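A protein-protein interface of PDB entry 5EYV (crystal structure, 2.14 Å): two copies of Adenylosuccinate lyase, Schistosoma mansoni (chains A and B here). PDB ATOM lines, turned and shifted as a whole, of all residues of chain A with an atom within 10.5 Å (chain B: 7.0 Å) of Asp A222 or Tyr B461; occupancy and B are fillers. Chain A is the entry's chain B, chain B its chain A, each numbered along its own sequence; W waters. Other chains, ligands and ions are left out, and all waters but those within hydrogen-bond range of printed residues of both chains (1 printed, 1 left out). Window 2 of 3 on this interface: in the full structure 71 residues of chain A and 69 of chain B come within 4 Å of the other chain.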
ATOM      1  N   GLN A  61      14.964 -10.340  12.166  1.00  0.00           N
ATOM      2  CA  GLN A  61      15.708  -9.433  11.299  1.00  0.00           C
ATOM      3  C   GLN A  61      15.140  -8.020  11.356  1.00  0.00           C
ATOM      4  O   GLN A  61      15.891  -7.041  11.297  1.00  0.00           O
ATOM      5  CB  GLN A  61      15.712  -9.964   9.868  1.00  0.00           C
ATOM      6  CG  GLN A  61      16.511 -11.242   9.709  1.00  0.00           C
ATOM      7  CD  GLN A  61      16.371 -11.854   8.335  1.00  0.00           C
ATOM      8  OE1 GLN A  61      15.392 -11.609   7.631  1.00  0.00           O
ATOM      9  NE2 GLN A  61      17.353 -12.656   7.943  1.00  0.00           N
ATOM     10  N   PHE A  66      16.738  -4.712  10.055  1.00  0.00           N
ATOM     11  CA  PHE A  66      16.560  -4.909   8.623  1.00  0.00           C
ATOM     12  C   PHE A  66      15.201  -4.388   8.168  1.00  0.00           C
ATOM     13  O   PHE A  66      14.205  -4.458   8.891  1.00  0.00           O
ATOM     14  CB  PHE A  66      16.712  -6.383   8.257  1.00  0.00           C
ATOM     15  CG  PHE A  66      17.762  -6.630   7.218  1.00  0.00           C
ATOM     16  CD1 PHE A  66      19.090  -6.764   7.581  1.00  0.00           C
ATOM     17  CD2 PHE A  66      17.424  -6.707   5.878  1.00  0.00           C
ATOM     18  CE1 PHE A  66      20.063  -6.979   6.627  1.00  0.00           C
ATOM     19  CE2 PHE A  66      18.392  -6.923   4.917  1.00  0.00           C
ATOM     20  CZ  PHE A  66      19.714  -7.056   5.292  1.00  0.00           C
ATOM     21  N   LEU A 119      15.129 -15.083   4.010  1.00  0.00           N
ATOM     22  CA  LEU A 119      16.207 -14.152   3.699  1.00  0.00           C
ATOM     23  C   LEU A 119      17.484 -14.523   4.442  1.00  0.00           C
ATOM     24  O   LEU A 119      17.510 -14.557   5.676  1.00  0.00           O
ATOM     25  CB  LEU A 119      15.775 -12.730   4.058  1.00  0.00           C
ATOM     26  CG  LEU A 119      16.783 -11.601   3.831  1.00  0.00           C
ATOM     27  CD1 LEU A 119      17.050 -11.397   2.347  1.00  0.00           C
ATOM     28  CD2 LEU A 119      16.290 -10.313   4.474  1.00  0.00           C
ATOM     29  N   GLY A 120      18.544 -14.802   3.684  1.00  0.00           N
ATOM     30  CA  GLY A 120      19.847 -15.095   4.239  1.00  0.00           C
ATOM     31  C   GLY A 120      20.013 -16.476   4.833  1.00  0.00           C
ATOM     32  O   GLY A 120      21.127 -16.823   5.247  1.00  0.00           O
ATOM     33  N   ALA A 121      18.957 -17.280   4.878  1.00  0.00           N
ATOM     34  CA  ALA A 121      19.004 -18.575   5.538  1.00  0.00           C
ATOM     35  C   ALA A 121      19.361 -19.684   4.551  1.00  0.00           C
ATOM     36  O   ALA A 121      19.311 -19.512   3.331  1.00  0.00           O
ATOM     37  CB  ALA A 121      17.666 -18.875   6.214  1.00  0.00           C
ATOM     38  N   LYS A 211      22.766 -21.024  11.411  1.00  0.00           N
ATOM     39  CA  LYS A 211      24.194 -21.297  11.370  1.00  0.00           C
ATOM     40  C   LYS A 211      24.792 -21.273   9.972  1.00  0.00           C
ATOM     41  O   LYS A 211      26.019 -21.208   9.846  1.00  0.00           O
ATOM     42  CB  LYS A 211      24.488 -22.660  12.016  1.00  0.00           C
ATOM     43  CG  LYS A 211      24.134 -22.710  13.484  1.00  0.00           C
ATOM     44  CD  LYS A 211      24.724 -21.514  14.211  1.00  0.00           C
ATOM     45  CE  LYS A 211      24.415 -21.577  15.686  1.00  0.00           C
ATOM     46  NZ  LYS A 211      24.785 -22.912  16.207  1.00  0.00           N
ATOM     47  N   GLY A 212      23.978 -21.323   8.929  1.00  0.00           N
ATOM     48  CA  GLY A 212      24.505 -21.281   7.584  1.00  0.00           C
ATOM     49  C   GLY A 212      24.808 -22.653   7.022  1.00  0.00           C
ATOM     50  O   GLY A 212      24.478 -23.698   7.594  1.00  0.00           O
ATOM     51  N   VAL A 214      27.682 -24.286   6.476  1.00  0.00           N
ATOM     52  CA  VAL A 214      28.674 -25.138   7.126  1.00  0.00           C
ATOM     53  C   VAL A 214      28.836 -24.744   8.588  1.00  0.00           C
ATOM     54  O   VAL A 214      29.821 -25.118   9.236  1.00  0.00           O
ATOM     55  CB  VAL A 214      30.027 -25.089   6.388  1.00  0.00           C
ATOM     56  CG1 VAL A 214      29.887 -25.648   4.977  1.00  0.00           C
ATOM     57  CG2 VAL A 214      30.574 -23.670   6.358  1.00  0.00           C
ATOM     58  N   THR A 216      29.171 -21.664   9.959  1.00  0.00           N
ATOM     59  CA  THR A 216      29.989 -20.494  10.247  1.00  0.00           C
ATOM     60  C   THR A 216      29.229 -19.179  10.127  1.00  0.00           C
ATOM     61  O   THR A 216      29.831 -18.118  10.320  1.00  0.00           O
ATOM     62  CB  THR A 216      31.207 -20.462   9.321  1.00  0.00           C
ATOM     63  OG1 THR A 216      30.769 -20.452   7.956  1.00  0.00           O
ATOM     64  CG2 THR A 216      32.092 -21.678   9.559  1.00  0.00           C
ATOM     65  N   GLN A 217      27.934 -19.220   9.802  1.00  0.00           N
ATOM     66  CA  GLN A 217      27.095 -18.022   9.726  1.00  0.00           C
ATOM     67  C   GLN A 217      27.649 -16.998   8.739  1.00  0.00           C
ATOM     68  O   GLN A 217      27.436 -15.792   8.893  1.00  0.00           O
ATOM     69  CB  GLN A 217      26.913 -17.387  11.109  1.00  0.00           C
ATOM     70  CG  GLN A 217      26.459 -18.366  12.178  1.00  0.00           C
ATOM     71  CD  GLN A 217      26.339 -17.724  13.543  1.00  0.00           C
ATOM     72  OE1 GLN A 217      27.326 -17.262  14.115  1.00  0.00           O
ATOM     73  NE2 GLN A 217      25.120 -17.684  14.071  1.00  0.00           N
ATOM     74  N   ALA A 218      28.358 -17.477   7.713  1.00  0.00           N
ATOM     75  CA  ALA A 218      28.997 -16.575   6.759  1.00  0.00           C
ATOM     76  C   ALA A 218      27.970 -15.781   5.960  1.00  0.00           C
ATOM     77  O   ALA A 218      28.210 -14.616   5.618  1.00  0.00           O
ATOM     78  CB  ALA A 218      29.907 -17.368   5.820  1.00  0.00           C
ATOM     79  N   SER A 219      26.824 -16.391   5.650  1.00  0.00           N
ATOM     80  CA  SER A 219      25.811 -15.688   4.870  1.00  0.00           C
ATOM     81  C   SER A 219      25.151 -14.584   5.688  1.00  0.00           C
ATOM     82  O   SER A 219      24.906 -13.486   5.172  1.00  0.00           O
ATOM     83  CB  SER A 219      24.766 -16.675   4.350  1.00  0.00           C
ATOM     84  OG  SER A 219      24.138 -17.364   5.416  1.00  0.00           O
ATOM     85  N   PHE A 220      24.859 -14.852   6.964  1.00  0.00           N
ATOM     86  CA  PHE A 220      24.248 -13.824   7.800  1.00  0.00           C
ATOM     87  C   PHE A 220      25.247 -12.738   8.179  1.00  0.00           C
ATOM     88  O   PHE A 220      24.858 -11.579   8.360  1.00  0.00           O
ATOM     89  CB  PHE A 220      23.633 -14.452   9.048  1.00  0.00           C
ATOM     90  CG  PHE A 220      22.341 -15.170   8.783  1.00  0.00           C
ATOM     91  CD1 PHE A 220      21.224 -14.474   8.355  1.00  0.00           C
ATOM     92  CD2 PHE A 220      22.241 -16.540   8.962  1.00  0.00           C
ATOM     93  CE1 PHE A 220      20.032 -15.126   8.106  1.00  0.00           C
ATOM     94  CE2 PHE A 220      21.051 -17.198   8.715  1.00  0.00           C
ATOM     95  CZ  PHE A 220      19.946 -16.490   8.288  1.00  0.00           C
ATOM     96  N   MET A 221      26.529 -13.087   8.305  1.00  0.00           N
ATOM     97  CA  MET A 221      27.553 -12.059   8.465  1.00  0.00           C
ATOM     98  C   MET A 221      27.563 -11.115   7.271  1.00  0.00           C
ATOM     99  O   MET A 221      27.710  -9.898   7.432  1.00  0.00           O
ATOM    100  CB  MET A 221      28.927 -12.705   8.653  1.00  0.00           C
ATOM    101  CG  MET A 221      29.170 -13.239  10.052  1.00  0.00           C
ATOM    102  SD  MET A 221      29.477 -11.920  11.242  1.00  0.00           S
ATOM    103  CE  MET A 221      31.070 -11.332  10.673  1.00  0.00           C
ATOM    104  N   ASP A 222      27.398 -11.660   6.064  1.00  0.00           N
ATOM    105  CA  ASP A 222      27.325 -10.818   4.875  1.00  0.00           C
ATOM    106  C   ASP A 222      26.056  -9.976   4.875  1.00  0.00           C
ATOM    107  O   ASP A 222      26.099  -8.782   4.557  1.00  0.00           O
ATOM    108  CB  ASP A 222      27.397 -11.681   3.616  1.00  0.00           C
ATOM    109  N   LEU A 223      24.920 -10.579   5.238  1.00  0.00           N
ATOM    110  CA  LEU A 223      23.663  -9.841   5.266  1.00  0.00           C
ATOM    111  C   LEU A 223      23.708  -8.693   6.264  1.00  0.00           C
ATOM    112  O   LEU A 223      23.049  -7.669   6.060  1.00  0.00           O
ATOM    113  CB  LEU A 223      22.508 -10.790   5.593  1.00  0.00           C
ATOM    114  CG  LEU A 223      21.093 -10.249   5.382  1.00  0.00           C
ATOM    115  CD1 LEU A 223      20.767 -10.161   3.898  1.00  0.00           C
ATOM    116  CD2 LEU A 223      20.064 -11.096   6.117  1.00  0.00           C
ATOM    117  N   PHE A 224      24.480  -8.837   7.342  1.00  0.00           N
ATOM    118  CA  PHE A 224      24.604  -7.801   8.358  1.00  0.00           C
ATOM    119  C   PHE A 224      25.888  -6.992   8.219  1.00  0.00           C
ATOM    120  O   PHE A 224      26.326  -6.369   9.191  1.00  0.00           O
ATOM    121  CB  PHE A 224      24.516  -8.416   9.755  1.00  0.00           C
ATOM    122  CG  PHE A 224      23.116  -8.741  10.184  1.00  0.00           C
ATOM    123  CD1 PHE A 224      22.274  -7.745  10.646  1.00  0.00           C
ATOM    124  CD2 PHE A 224      22.643 -10.041  10.125  1.00  0.00           C
ATOM    125  CE1 PHE A 224      20.983  -8.037  11.043  1.00  0.00           C
ATOM    126  CE2 PHE A 224      21.352 -10.341  10.521  1.00  0.00           C
ATOM    127  CZ  PHE A 224      20.521  -9.337  10.981  1.00  0.00           C
ATOM    128  N   GLN A 225      26.500  -6.996   7.032  1.00  0.00           N
ATOM    129  CA  GLN A 225      27.702  -6.207   6.752  1.00  0.00           C
ATOM    130  C   GLN A 225      28.823  -6.505   7.746  1.00  0.00           C
ATOM    131  O   GLN A 225      29.612  -5.623   8.098  1.00  0.00           O
ATOM    132  CB  GLN A 225      27.386  -4.708   6.729  1.00  0.00           C
ATOM    133  N   GLY A 226      28.897  -7.750   8.211  1.00  0.00           N
ATOM    134  CA  GLY A 226      29.987  -8.166   9.071  1.00  0.00           C
ATOM    135  C   GLY A 226      29.838  -7.828  10.536  1.00  0.00           C
ATOM    136  O   GLY A 226      30.823  -7.907  11.277  1.00  0.00           O
ATOM    137  N   ASP A 227      28.641  -7.459  10.985  1.00  0.00           N
ATOM    138  CA  ASP A 227      28.421  -7.118  12.389  1.00  0.00           C
ATOM    139  C   ASP A 227      28.304  -8.414  13.182  1.00  0.00           C
ATOM    140  O   ASP A 227      27.269  -9.085  13.151  1.00  0.00           O
ATOM    141  CB  ASP A 227      27.178  -6.249  12.541  1.00  0.00           C
ATOM    142  CG  ASP A 227      27.092  -5.580  13.903  1.00  0.00           C
ATOM    143  OD1 ASP A 227      27.337  -6.253  14.927  1.00  0.00           O
ATOM    144  OD2 ASP A 227      26.778  -4.372  13.952  1.00  0.00           O
ATOM    145  N   HIS A 228      29.374  -8.766  13.902  1.00  0.00           N
ATOM    146  CA  HIS A 228      29.378 -10.000  14.684  1.00  0.00           C
ATOM    147  C   HIS A 228      28.264 -10.007  15.723  1.00  0.00           C
ATOM    148  O   HIS A 228      27.611 -11.035  15.936  1.00  0.00           O
ATOM    149  CB  HIS A 228      30.735 -10.190  15.367  1.00  0.00           C
ATOM    150  CG  HIS A 228      31.824 -10.648  14.448  1.00  0.00           C
ATOM    151  ND1 HIS A 228      32.163 -11.976  14.302  1.00  0.00           N
ATOM    152  CD2 HIS A 228      32.660  -9.956  13.638  1.00  0.00           C
ATOM    153  CE1 HIS A 228      33.157 -12.083  13.437  1.00  0.00           C
ATOM    154  NE2 HIS A 228      33.476 -10.872  13.019  1.00  0.00           N
ATOM    155  N   LYS A 230      25.348  -8.516  15.718  1.00  0.00           N
ATOM    156  CA  LYS A 230      24.032  -8.726  15.122  1.00  0.00           C
ATOM    157  C   LYS A 230      23.782 -10.206  14.854  1.00  0.00           C
ATOM    158  O   LYS A 230      22.704 -10.731  15.159  1.00  0.00           O
ATOM    159  CB  LYS A 230      23.901  -7.922  13.828  1.00  0.00           C
ATOM    160  CG  LYS A 230      23.035  -6.672  13.928  1.00  0.00           C
ATOM    161  CD  LYS A 230      23.767  -5.532  14.610  1.00  0.00           C
ATOM    162  CE  LYS A 230      23.225  -4.180  14.162  1.00  0.00           C
ATOM    163  NZ  LYS A 230      21.784  -4.003  14.496  1.00  0.00           N
ATOM    164  N   VAL A 231      24.770 -10.896  14.277  1.00  0.00           N
ATOM    165  CA  VAL A 231      24.613 -12.317  13.978  1.00  0.00           C
ATOM    166  C   VAL A 231      24.451 -13.117  15.264  1.00  0.00           C
ATOM    167  O   VAL A 231      23.654 -14.061  15.330  1.00  0.00           O
ATOM    168  CB  VAL A 231      25.801 -12.819  13.136  1.00  0.00           C
ATOM    169  CG1 VAL A 231      25.755 -14.334  12.990  1.00  0.00           C
ATOM    170  CG2 VAL A 231      25.788 -12.155  11.767  1.00  0.00           C
ATOM    171  N   LEU A 234      20.986 -12.529  16.422  1.00  0.00           N
ATOM    172  CA  LEU A 234      20.063 -13.258  15.555  1.00  0.00           C
ATOM    173  C   LEU A 234      19.824 -14.671  16.071  1.00  0.00           C
ATOM    174  O   LEU A 234      18.683 -15.143  16.130  1.00  0.00           O
ATOM    175  CB  LEU A 234      20.610 -13.294  14.127  1.00  0.00           C
ATOM    176  CG  LEU A 234      19.912 -14.229  13.134  1.00  0.00           C
ATOM    177  CD1 LEU A 234      18.507 -13.746  12.821  1.00  0.00           C
ATOM    178  CD2 LEU A 234      20.727 -14.359  11.858  1.00  0.00           C
ATOM    179  N   ILE B 164      42.794 -21.563   7.367  1.00  0.00           N
ATOM    180  CA  ILE B 164      41.657 -21.635   6.458  1.00  0.00           C
ATOM    181  C   ILE B 164      41.781 -22.864   5.569  1.00  0.00           C
ATOM    182  O   ILE B 164      42.853 -23.159   5.022  1.00  0.00           O
ATOM    183  CB  ILE B 164      41.557 -20.349   5.619  1.00  0.00           C
ATOM    184  CG1 ILE B 164      41.540 -19.121   6.531  1.00  0.00           C
ATOM    185  CG2 ILE B 164      40.311 -20.379   4.747  1.00  0.00           C
ATOM    186  CD1 ILE B 164      41.418 -17.809   5.788  1.00  0.00           C
ATOM    187  N   PRO B 454      37.470  -6.898  -3.402  1.00  0.00           N
ATOM    188  CA  PRO B 454      38.555  -7.233  -2.458  1.00  0.00           C
ATOM    189  C   PRO B 454      38.084  -7.902  -1.176  1.00  0.00           C
ATOM    190  O   PRO B 454      38.826  -8.711  -0.603  1.00  0.00           O
ATOM    191  CB  PRO B 454      39.202  -5.869  -2.179  1.00  0.00           C
ATOM    192  CG  PRO B 454      38.967  -5.102  -3.415  1.00  0.00           C
ATOM    193  CD  PRO B 454      37.599  -5.512  -3.887  1.00  0.00           C
ATOM    194  N   THR B 455      36.872  -7.598  -0.710  1.00  0.00           N
ATOM    195  CA  THR B 455      36.313  -8.267   0.458  1.00  0.00           C
ATOM    196  C   THR B 455      35.541  -9.526   0.081  1.00  0.00           C
ATOM    197  O   THR B 455      35.650 -10.547   0.770  1.00  0.00           O
ATOM    198  CB  THR B 455      35.401  -7.309   1.230  1.00  0.00           C
ATOM    199  OG1 THR B 455      36.136  -6.131   1.584  1.00  0.00           O
ATOM    200  CG2 THR B 455      34.878  -7.971   2.497  1.00  0.00           C
ATOM    201  N   VAL B 456      34.765  -9.468  -1.006  1.00  0.00           N
ATOM    202  CA  VAL B 456      34.018 -10.636  -1.469  1.00  0.00           C
ATOM    203  C   VAL B 456      34.957 -11.806  -1.728  1.00  0.00           C
ATOM    204  O   VAL B 456      34.634 -12.962  -1.430  1.00  0.00           O
ATOM    205  CB  VAL B 456      33.198 -10.274  -2.724  1.00  0.00           C
ATOM    206  CG1 VAL B 456      32.773 -11.528  -3.474  1.00  0.00           C
ATOM    207  CG2 VAL B 456      31.982  -9.444  -2.343  1.00  0.00           C
ATOM    208  N   LEU B 457      36.139 -11.525  -2.267  1.00  0.00           N
ATOM    209  CA  LEU B 457      37.118 -12.549  -2.605  1.00  0.00           C
ATOM    210  C   LEU B 457      38.069 -12.872  -1.459  1.00  0.00           C
ATOM    211  O   LEU B 457      38.963 -13.705  -1.634  1.00  0.00           O
ATOM    212  CB  LEU B 457      37.927 -12.116  -3.834  1.00  0.00           C
ATOM    213  CG  LEU B 457      37.422 -12.497  -5.229  1.00  0.00           C
ATOM    214  CD1 LEU B 457      35.915 -12.338  -5.361  1.00  0.00           C
ATOM    215  CD2 LEU B 457      38.134 -11.655  -6.274  1.00  0.00           C
ATOM    216  N   ASP B 458      37.900 -12.244  -0.301  1.00  0.00           N
ATOM    217  CA  ASP B 458      38.800 -12.476   0.823  1.00  0.00           C
ATOM    218  C   ASP B 458      38.421 -13.771   1.532  1.00  0.00           C
ATOM    219  O   ASP B 458      37.302 -13.874   2.048  1.00  0.00           O
ATOM    220  CB  ASP B 458      38.744 -11.306   1.799  1.00  0.00           C
ATOM    221  CG  ASP B 458      39.900 -11.305   2.787  1.00  0.00           C
ATOM    222  OD1 ASP B 458      40.557 -12.353   2.955  1.00  0.00           O
ATOM    223  OD2 ASP B 458      40.151 -10.247   3.402  1.00  0.00           O
ATOM    224  N   PRO B 459      39.307 -14.772   1.579  1.00  0.00           N
ATOM    225  CA  PRO B 459      38.972 -16.001   2.322  1.00  0.00           C
ATOM    226  C   PRO B 459      38.721 -15.756   3.800  1.00  0.00           C
ATOM    227  O   PRO B 459      37.873 -16.430   4.399  1.00  0.00           O
ATOM    228  CB  PRO B 459      40.201 -16.894   2.092  1.00  0.00           C
ATOM    229  CG  PRO B 459      40.838 -16.358   0.847  1.00  0.00           C
ATOM    230  CD  PRO B 459      40.603 -14.878   0.888  1.00  0.00           C
ATOM    231  N   SER B 460      39.437 -14.802   4.405  1.00  0.00           N
ATOM    232  CA  SER B 460      39.185 -14.450   5.797  1.00  0.00           C
ATOM    233  C   SER B 460      37.780 -13.905   6.002  1.00  0.00           C
ATOM    234  O   SER B 460      37.275 -13.920   7.131  1.00  0.00           O
ATOM    235  CB  SER B 460      40.215 -13.426   6.276  1.00  0.00           C
ATOM    236  OG  SER B 460      41.536 -13.907   6.098  1.00  0.00           O
ATOM    237  N   TYR B 461      37.142 -13.417   4.938  1.00  0.00           N
ATOM    238  CA  TYR B 461      35.754 -12.984   5.019  1.00  0.00           C
ATOM    239  C   TYR B 461      34.799 -14.155   4.817  1.00  0.00           C
ATOM    240  O   TYR B 461      33.761 -14.237   5.485  1.00  0.00           O
ATOM    241  CB  TYR B 461      35.496 -11.889   3.982  1.00  0.00           C
ATOM    242  CG  TYR B 461      34.085 -11.348   3.974  1.00  0.00           C
ATOM    243  CD1 TYR B 461      33.697 -10.356   4.865  1.00  0.00           C
ATOM    244  CD2 TYR B 461      33.144 -11.816   3.065  1.00  0.00           C
ATOM    245  CE1 TYR B 461      32.412  -9.852   4.858  1.00  0.00           C
ATOM    246  CE2 TYR B 461      31.855 -11.318   3.051  1.00  0.00           C
ATOM    247  CZ  TYR B 461      31.495 -10.337   3.949  1.00  0.00           C
ATOM    248  OH  TYR B 461      30.215  -9.836   3.941  1.00  0.00           O
ATOM    249  N   MET B 462      35.143 -15.078   3.912  1.00  0.00           N
ATOM    250  CA  MET B 462      34.244 -16.177   3.577  1.00  0.00           C
ATOM    251  C   MET B 462      34.024 -17.136   4.739  1.00  0.00           C
ATOM    252  O   MET B 462      32.996 -17.823   4.770  1.00  0.00           O
ATOM    253  CB  MET B 462      34.785 -16.954   2.377  1.00  0.00           C
ATOM    254  CG  MET B 462      35.117 -16.099   1.167  1.00  0.00           C
ATOM    255  SD  MET B 462      35.642 -17.110  -0.231  1.00  0.00           S
ATOM    256  CE  MET B 462      36.338 -15.868  -1.311  1.00  0.00           C
ATOM    257  N   ILE B 463      34.960 -17.205   5.693  1.00  0.00           N
ATOM    258  CA  ILE B 463      34.835 -18.147   6.805  1.00  0.00           C
ATOM    259  C   ILE B 463      33.848 -17.690   7.866  1.00  0.00           C
ATOM    260  O   ILE B 463      33.628 -18.420   8.841  1.00  0.00           O
ATOM    261  CB  ILE B 463      36.201 -18.407   7.472  1.00  0.00           C
ATOM    262  CG1 ILE B 463      36.802 -17.102   7.999  1.00  0.00           C
ATOM    263  CG2 ILE B 463      37.153 -19.084   6.495  1.00  0.00           C
ATOM    264  CD1 ILE B 463      38.151 -17.280   8.666  1.00  0.00           C
ATOM    265  N   GLY B 464      33.251 -16.511   7.711  1.00  0.00           N
ATOM    266  CA  GLY B 464      32.239 -16.073   8.661  1.00  0.00           C
ATOM    267  C   GLY B 464      32.816 -15.887  10.052  1.00  0.00           C
ATOM    268  O   GLY B 464      33.855 -15.245  10.238  1.00  0.00           O
ATOM    269  N   ARG B 465      32.135 -16.459  11.047  1.00  0.00           N
ATOM    270  CA  ARG B 465      32.548 -16.367  12.443  1.00  0.00           C
ATOM    271  C   ARG B 465      33.328 -17.595  12.902  1.00  0.00           C
ATOM    272  O   ARG B 465      33.334 -17.908  14.096  1.00  0.00           O
ATOM    273  CB  ARG B 465      31.333 -16.157  13.348  1.00  0.00           C
ATOM    274  CG  ARG B 465      30.421 -15.014  12.937  1.00  0.00           C
ATOM    275  CD  ARG B 465      29.486 -14.606  14.070  1.00  0.00           C
ATOM    276  NE  ARG B 465      30.211 -13.949  15.155  1.00  0.00           N
ATOM    277  CZ  ARG B 465      30.493 -14.513  16.325  1.00  0.00           C
ATOM    278  NH1 ARG B 465      30.100 -15.753  16.581  1.00  0.00           N
ATOM    279  NH2 ARG B 465      31.165 -13.831  17.246  1.00  0.00           N
HETATM  280  O   HOH W   1      31.956 -20.329   5.860  1.00  0.00           O
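The backbone carbonyl oxygen (O) of Thr A216 is in hydrogen-bond range of the backbone NH (N) of Arg B465, at 2.9 Å.
ND1 of His A228 lies within hydrogen-bond range of NE of Arg B465, at 2.9 Å.
The backbone NH (N) of Thr A216 is in hydrogen-bond range of the backbone carbonyl oxygen (O) of Lys A211, at 3.2 Å.
The backbone carbonyl oxygen (O) of Lys A211 is in hydrogen-bond range of the backbone NH (N) of Gln A217, 2.8 Å away.
The backbone carbonyl oxygen (O) of Met A221 is in hydrogen-bond range of the backbone NH (N) of Gly A226 (2.6 Å).
Among the printed residues, merely in contact across the chains: Thr A216 with Ile B463, Thr A216 with Gly B464, Gln A217 with Arg B465, Ala A218 with Met B462, Ala A218 with Gly B464, Met A221 with Arg B465, Asp A222 with Tyr B461 and Val A231 with Arg B465.
Of the printed residues of chain B, Gln A217 touches Arg B465 (3.4 Å).
Of the printed residues of chain B, Ala A218 touches Met B462 and Gly B464.
Of chain B, only Tyr B461 (3.2 Å) comes within 4 Å of Asp A222.
Val B456 touches none of the printed residues of chain A.
Asp B458 touches none of the printed residues of chain A.
No residue of chain A comes within 4 Å of Pro B459.
No residue of chain A comes within 4 Å of Ser B460.
Tyr B461 touches one residue of chain A.
Of the printed residues of chain A, Met B462 touches Ala A218.
Printed residues of chain A within 4 Å of Gly B464: Thr A216 and Ala A218.
Of the printed residues of chain A, Arg B465 touches Thr A216 (2.9 Å), Gln A217 (3.4 Å), Met A221 (3.6 Å), His A228 (2.9 Å) and Val A231 (3.9 Å).
The nearest printed residue of chain B that does not touch Asp A222 is Gly B464 (7.0 Å).
The nearest residue of chain A that does not touch Tyr B461 is Met A221 (4.3 Å).
Of the 24 printed residues of chain A, 7 touch a printed residue of chain B.
Hydrophobic or aromatic side chains of chain B within 4 Å of the printed part of chain A: Tyr B461.
Among the printed residues, 10 pairs touch across the chains.
Among the printed residues, no Asp or Glu carboxylate lies within 4 Å of a Lys or Arg side-chain nitrogen of the other chain.
No position is printed for both chains.
Of the 10 pairs that touch across the chains among the printed residues, none has its exchanged pair printed and touching as well.
Water W1 lies within hydrogen-bond range of OG1 of Thr A216 (2.4 Å) and O of Met B462 (2.9 Å).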
